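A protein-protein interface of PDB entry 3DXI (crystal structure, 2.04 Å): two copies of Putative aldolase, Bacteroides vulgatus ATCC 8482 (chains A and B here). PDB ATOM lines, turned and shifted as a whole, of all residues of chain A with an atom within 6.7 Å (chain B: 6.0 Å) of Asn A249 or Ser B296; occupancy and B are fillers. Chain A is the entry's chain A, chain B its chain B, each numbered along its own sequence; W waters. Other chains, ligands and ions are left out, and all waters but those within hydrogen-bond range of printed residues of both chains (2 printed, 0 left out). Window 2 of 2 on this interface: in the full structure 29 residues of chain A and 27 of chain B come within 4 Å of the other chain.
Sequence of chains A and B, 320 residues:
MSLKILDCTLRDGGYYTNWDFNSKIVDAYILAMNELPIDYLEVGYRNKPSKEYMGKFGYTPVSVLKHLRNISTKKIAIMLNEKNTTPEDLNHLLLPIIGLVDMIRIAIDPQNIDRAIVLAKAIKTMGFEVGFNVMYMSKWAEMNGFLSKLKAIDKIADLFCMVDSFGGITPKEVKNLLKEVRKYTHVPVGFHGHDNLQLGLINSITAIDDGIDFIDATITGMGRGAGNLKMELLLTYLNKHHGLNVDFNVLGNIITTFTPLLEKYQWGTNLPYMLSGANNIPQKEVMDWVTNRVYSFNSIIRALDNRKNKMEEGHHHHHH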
ATOM      1  N   VAL A 246       6.559 -22.262  18.521  1.00  0.00           N
ATOM      2  CA  VAL A 246       7.473 -21.133  18.374  1.00  0.00           C
ATOM      3  C   VAL A 246       8.776 -21.520  17.679  1.00  0.00           C
ATOM      4  O   VAL A 246       9.349 -22.576  17.962  1.00  0.00           O
ATOM      5  CB  VAL A 246       7.840 -20.537  19.754  1.00  0.00           C
ATOM      6  CG1 VAL A 246       8.914 -19.461  19.600  1.00  0.00           C
ATOM      7  CG2 VAL A 246       6.612 -19.958  20.411  1.00  0.00           C
ATOM      8  N   ASP A 247       9.246 -20.662  16.775  1.00  0.00           N
ATOM      9  CA  ASP A 247      10.514 -20.903  16.088  1.00  0.00           C
ATOM     10  C   ASP A 247      11.561 -20.189  16.932  1.00  0.00           C
ATOM     11  O   ASP A 247      11.766 -18.982  16.800  1.00  0.00           O
ATOM     12  CB  ASP A 247      10.531 -20.304  14.684  1.00  0.00           C
ATOM     13  CG  ASP A 247      11.829 -20.602  13.946  1.00  0.00           C
ATOM     14  OD1 ASP A 247      12.860 -20.806  14.618  1.00  0.00           O
ATOM     15  OD2 ASP A 247      11.825 -20.626  12.701  1.00  0.00           O
ATOM     16  N   PHE A 248      12.212 -20.947  17.801  1.00  0.00           N
ATOM     17  CA  PHE A 248      13.214 -20.396  18.696  1.00  0.00           C
ATOM     18  C   PHE A 248      14.493 -19.938  18.010  1.00  0.00           C
ATOM     19  O   PHE A 248      15.225 -19.109  18.553  1.00  0.00           O
ATOM     20  CB  PHE A 248      13.510 -21.418  19.787  1.00  0.00           C
ATOM     21  CG  PHE A 248      12.381 -21.586  20.764  1.00  0.00           C
ATOM     22  CD1 PHE A 248      12.167 -20.639  21.759  1.00  0.00           C
ATOM     23  CD2 PHE A 248      11.509 -22.670  20.669  1.00  0.00           C
ATOM     24  CE1 PHE A 248      11.103 -20.768  22.645  1.00  0.00           C
ATOM     25  CE2 PHE A 248      10.438 -22.810  21.552  1.00  0.00           C
ATOM     26  CZ  PHE A 248      10.234 -21.858  22.542  1.00  0.00           C
ATOM     27  N   ASN A 249      14.763 -20.472  16.822  1.00  0.00           N
ATOM     28  CA  ASN A 249      15.956 -20.079  16.086  1.00  0.00           C
ATOM     29  C   ASN A 249      15.796 -18.608  15.730  1.00  0.00           C
ATOM     30  O   ASN A 249      16.711 -17.808  15.944  1.00  0.00           O
ATOM     31  CB  ASN A 249      16.126 -20.933  14.822  1.00  0.00           C
ATOM     32  CG  ASN A 249      16.636 -22.338  15.131  1.00  0.00           C
ATOM     33  OD1 ASN A 249      16.658 -22.763  16.285  1.00  0.00           O
ATOM     34  ND2 ASN A 249      17.041 -23.068  14.093  1.00  0.00           N
ATOM     35  N   VAL A 250      14.622 -18.259  15.205  1.00  0.00           N
ATOM     36  CA  VAL A 250      14.313 -16.877  14.846  1.00  0.00           C
ATOM     37  C   VAL A 250      14.286 -16.004  16.104  1.00  0.00           C
ATOM     38  O   VAL A 250      14.801 -14.892  16.102  1.00  0.00           O
ATOM     39  CB  VAL A 250      12.932 -16.769  14.138  1.00  0.00           C
ATOM     40  CG1 VAL A 250      12.515 -15.307  14.014  1.00  0.00           C
ATOM     41  CG2 VAL A 250      13.005 -17.408  12.746  1.00  0.00           C
ATOM     42  N   LEU A 251      13.686 -16.510  17.177  1.00  0.00           N
ATOM     43  CA  LEU A 251      13.606 -15.756  18.420  1.00  0.00           C
ATOM     44  C   LEU A 251      15.015 -15.403  18.909  1.00  0.00           C
ATOM     45  O   LEU A 251      15.286 -14.262  19.280  1.00  0.00           O
ATOM     46  CB  LEU A 251      12.852 -16.569  19.483  1.00  0.00           C
ATOM     47  CG  LEU A 251      12.467 -15.866  20.790  1.00  0.00           C
ATOM     48  CD1 LEU A 251      11.723 -14.565  20.496  1.00  0.00           C
ATOM     49  CD2 LEU A 251      11.588 -16.803  21.612  1.00  0.00           C
ATOM     50  N   GLY A 252      15.912 -16.383  18.904  1.00  0.00           N
ATOM     51  CA  GLY A 252      17.275 -16.131  19.333  1.00  0.00           C
ATOM     52  C   GLY A 252      17.977 -15.126  18.434  1.00  0.00           C
ATOM     53  O   GLY A 252      18.730 -14.274  18.909  1.00  0.00           O
ATOM     54  N   ASN A 253      17.737 -15.217  17.128  1.00  0.00           N
ATOM     55  CA  ASN A 253      18.369 -14.292  16.199  1.00  0.00           C
ATOM     56  C   ASN A 253      17.870 -12.859  16.356  1.00  0.00           C
ATOM     57  O   ASN A 253      18.654 -11.918  16.256  1.00  0.00           O
ATOM     58  CB  ASN A 253      18.170 -14.741  14.749  1.00  0.00           C
ATOM     59  CG  ASN A 253      18.892 -16.041  14.435  1.00  0.00           C
ATOM     60  OD1 ASN A 253      19.891 -16.378  15.076  1.00  0.00           O
ATOM     61  ND2 ASN A 253      18.397 -16.773  13.442  1.00  0.00           N
ATOM     62  N   ILE A 254      16.575 -12.683  16.602  1.00  0.00           N
ATOM     63  CA  ILE A 254      16.053 -11.335  16.745  1.00  0.00           C
ATOM     64  C   ILE A 254      16.524 -10.729  18.070  1.00  0.00           C
ATOM     65  O   ILE A 254      16.693  -9.516  18.180  1.00  0.00           O
ATOM     66  CB  ILE A 254      14.499 -11.299  16.617  1.00  0.00           C
ATOM     67  CG1 ILE A 254      14.030  -9.848  16.470  1.00  0.00           C
ATOM     68  CG2 ILE A 254      13.835 -11.943  17.827  1.00  0.00           C
ATOM     69  CD1 ILE A 254      14.631  -9.125  15.268  1.00  0.00           C
ATOM     70  N   TYR B 295      23.582 -27.869  18.300  1.00  0.00           N
ATOM     71  CA  TYR B 295      22.142 -27.723  18.509  1.00  0.00           C
ATOM     72  C   TYR B 295      21.621 -26.299  18.387  1.00  0.00           C
ATOM     73  O   TYR B 295      22.073 -25.401  19.099  1.00  0.00           O
ATOM     74  CB  TYR B 295      21.725 -28.223  19.899  1.00  0.00           C
ATOM     75  CG  TYR B 295      21.550 -29.718  20.029  1.00  0.00           C
ATOM     76  CD1 TYR B 295      21.049 -30.478  18.978  1.00  0.00           C
ATOM     77  CD2 TYR B 295      21.852 -30.367  21.223  1.00  0.00           C
ATOM     78  CE1 TYR B 295      20.853 -31.854  19.112  1.00  0.00           C
ATOM     79  CE2 TYR B 295      21.658 -31.739  21.369  1.00  0.00           C
ATOM     80  CZ  TYR B 295      21.159 -32.474  20.311  1.00  0.00           C
ATOM     81  OH  TYR B 295      20.964 -33.829  20.453  1.00  0.00           O
ATOM     82  N   SER B 296      20.664 -26.098  17.489  1.00  0.00           N
ATOM     83  CA  SER B 296      20.038 -24.793  17.350  1.00  0.00           C
ATOM     84  C   SER B 296      18.978 -24.830  18.454  1.00  0.00           C
ATOM     85  O   SER B 296      18.707 -25.889  19.019  1.00  0.00           O
ATOM     86  CB  SER B 296      19.364 -24.655  15.981  1.00  0.00           C
ATOM     87  OG  SER B 296      18.307 -25.594  15.832  1.00  0.00           O
ATOM     88  N   PHE B 297      18.374 -23.698  18.778  1.00  0.00           N
ATOM     89  CA  PHE B 297      17.363 -23.716  19.825  1.00  0.00           C
ATOM     90  C   PHE B 297      16.212 -24.671  19.505  1.00  0.00           C
ATOM     91  O   PHE B 297      15.725 -25.369  20.395  1.00  0.00           O
ATOM     92  CB  PHE B 297      16.848 -22.296  20.088  1.00  0.00           C
ATOM     93  CG  PHE B 297      17.852 -21.411  20.779  1.00  0.00           C
ATOM     94  CD1 PHE B 297      18.202 -20.179  20.241  1.00  0.00           C
ATOM     95  CD2 PHE B 297      18.470 -21.825  21.954  1.00  0.00           C
ATOM     96  CE1 PHE B 297      19.160 -19.369  20.867  1.00  0.00           C
ATOM     97  CE2 PHE B 297      19.425 -21.027  22.586  1.00  0.00           C
ATOM     98  CZ  PHE B 297      19.772 -19.796  22.039  1.00  0.00           C
ATOM     99  N   ASN B 298      15.781 -24.724  18.246  1.00  0.00           N
ATOM    100  CA  ASN B 298      14.685 -25.626  17.880  1.00  0.00           C
ATOM    101  C   ASN B 298      15.070 -27.096  18.032  1.00  0.00           C
ATOM    102  O   ASN B 298      14.231 -27.932  18.367  1.00  0.00           O
ATOM    103  CB  ASN B 298      14.215 -25.382  16.443  1.00  0.00           C
ATOM    104  CG  ASN B 298      13.497 -24.057  16.281  1.00  0.00           C
ATOM    105  OD1 ASN B 298      12.784 -23.613  17.182  1.00  0.00           O
ATOM    106  ND2 ASN B 298      13.667 -23.429  15.125  1.00  0.00           N
ATOM    107  N   SER B 299      16.336 -27.411  17.785  1.00  0.00           N
ATOM    108  CA  SER B 299      16.798 -28.787  17.905  1.00  0.00           C
ATOM    109  C   SER B 299      16.845 -29.216  19.364  1.00  0.00           C
ATOM    110  O   SER B 299      16.598 -30.380  19.685  1.00  0.00           O
ATOM    111  CB  SER B 299      18.179 -28.943  17.271  1.00  0.00           C
ATOM    112  OG  SER B 299      18.098 -28.772  15.870  1.00  0.00           O
ATOM    113  N   ILE B 300      17.173 -28.279  20.246  1.00  0.00           N
ATOM    114  CA  ILE B 300      17.225 -28.583  21.669  1.00  0.00           C
ATOM    115  C   ILE B 300      15.823 -28.968  22.128  1.00  0.00           C
ATOM    116  O   ILE B 300      15.651 -29.850  22.970  1.00  0.00           O
ATOM    117  CB  ILE B 300      17.730 -27.365  22.488  1.00  0.00           C
ATOM    118  CG1 ILE B 300      19.214 -27.130  22.189  1.00  0.00           C
ATOM    119  CG2 ILE B 300      17.509 -27.602  23.987  1.00  0.00           C
ATOM    120  CD1 ILE B 300      19.858 -26.016  23.002  1.00  0.00           C
ATOM    121  N   ILE B 301      14.821 -28.319  21.545  1.00  0.00           N
ATOM    122  CA  ILE B 301      13.438 -28.580  21.895  1.00  0.00           C
ATOM    123  C   ILE B 301      12.831 -29.764  21.163  1.00  0.00           C
ATOM    124  O   ILE B 301      12.026 -30.506  21.733  1.00  0.00           O
ATOM    125  CB  ILE B 301      12.567 -27.334  21.651  1.00  0.00           C
ATOM    126  CG1 ILE B 301      12.869 -26.305  22.740  1.00  0.00           C
ATOM    127  CG2 ILE B 301      11.082 -27.709  21.615  1.00  0.00           C
ATOM    128  CD1 ILE B 301      11.779 -25.303  22.957  1.00  0.00           C
ATOM    129  N   ARG B 302      13.209 -29.945  19.902  1.00  0.00           N
ATOM    130  CA  ARG B 302      12.679 -31.054  19.126  1.00  0.00           C
ATOM    131  C   ARG B 302      12.977 -32.359  19.846  1.00  0.00           C
ATOM    132  O   ARG B 302      12.129 -33.253  19.904  1.00  0.00           O
ATOM    133  CB  ARG B 302      13.287 -31.056  17.720  1.00  0.00           C
ATOM    134  CG  ARG B 302      12.819 -32.204  16.824  1.00  0.00           C
ATOM    135  CD  ARG B 302      12.763 -31.775  15.358  1.00  0.00           C
ATOM    136  NE  ARG B 302      13.748 -30.744  15.033  1.00  0.00           N
ATOM    137  CZ  ARG B 302      15.058 -30.853  15.246  1.00  0.00           C
ATOM    138  NH1 ARG B 302      15.565 -31.953  15.791  1.00  0.00           N
ATOM    139  NH2 ARG B 302      15.867 -29.859  14.905  1.00  0.00           N
HETATM  140  O   HOH W   1      10.243 -25.280  18.613  1.00  0.00           O
HETATM  141  O   HOH W   2      19.622 -21.535  17.587  1.00  0.00           O
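The side-chain amide nitrogen (ND2) of Asn B298 sits at hydrogen-bond distance from the side-chain carboxylate (OD1) of Asp A247. The side-chain amide oxygen (OD1) of Asn B298 is in hydrogen-bond range of the backbone NH (N) of Phe A248 (2.8 Å). The side-chain amide oxygen of Asn A249 sits at hydrogen-bond distance from the side-chain hydroxyl of Ser B296. The backbone NH of Phe B297 sits at hydrogen-bond distance from the side-chain amide oxygen of Asn A249. The backbone NH of Asn B298 sits at hydrogen-bond distance from the side-chain amide oxygen of Asn A249 (2.9 Å).
OD1 of Asp A247 is in hydrogen-bond range of N of Asn A249 (2.9 Å). The side-chain carboxylate (OD1) of Asp A247 lies within hydrogen-bond range of the backbone NH (N) of Val A250. O of Asn A249 sits close to ND2 of Asn A253, at 3.2 Å. The side-chain hydroxyl of Ser B296 lies within hydrogen-bond range of the side-chain hydroxyl of Ser B299 (3.2 Å).
O of Val A246 touches OD1 of Asn B298, at 3.7 Å. CB of Phe A248 touches CB of Phe B297 (3.5 Å). Phe A248 touches Ile B301 (CE2 to CD1, 3.2 Å).
Of the printed residues of chain B, Val A246 touches Asn B298. Of the printed residues of chain B, Asp A247 touches Asn B298 (2.8 Å). Printed residues of chain B within 4 Å of Asn A249: Ser B296, Phe B297 and Asn B298. Val A250 touches none of the printed residues of chain B. Leu A251 touches none of the printed residues of chain B. Ser B296 touches just one residue of chain A: Asn A249. Printed residues of chain A within 4 Å of Phe B297: Phe A248 (3.5 Å) and Asn A249 (3.2 Å). Of the printed residues of chain A, Asn B298 touches Val A246, Asp A247, Phe A248 and Asn A249.
Printed residues of chain B that touch a printed residue of chain A: Ser B296, Phe B297, Asn B298 and Ile B301. Hydrophobic or aromatic side chains of chain A that line the printed part of chain B: Phe A248. Among the printed residues, no Asp or Glu carboxylate lies within 4 Å of a Lys or Arg side-chain nitrogen of the other chain.
No position is printed for both chains. Of the 8 pairs that touch across the chains among the printed residues, none has its exchanged pair printed and touching as well.
Water W2 lies within hydrogen-bond range of the backbone NH of Phe B297 (2.8 Å) and the side-chain amide oxygen of Asn A249 (3.5 Å). Water W1 lies within hydrogen-bond range of the backbone carbonyl oxygen of Val A246 (2.9 Å) and the side-chain amide oxygen of Asn B298 (3.4 Å).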
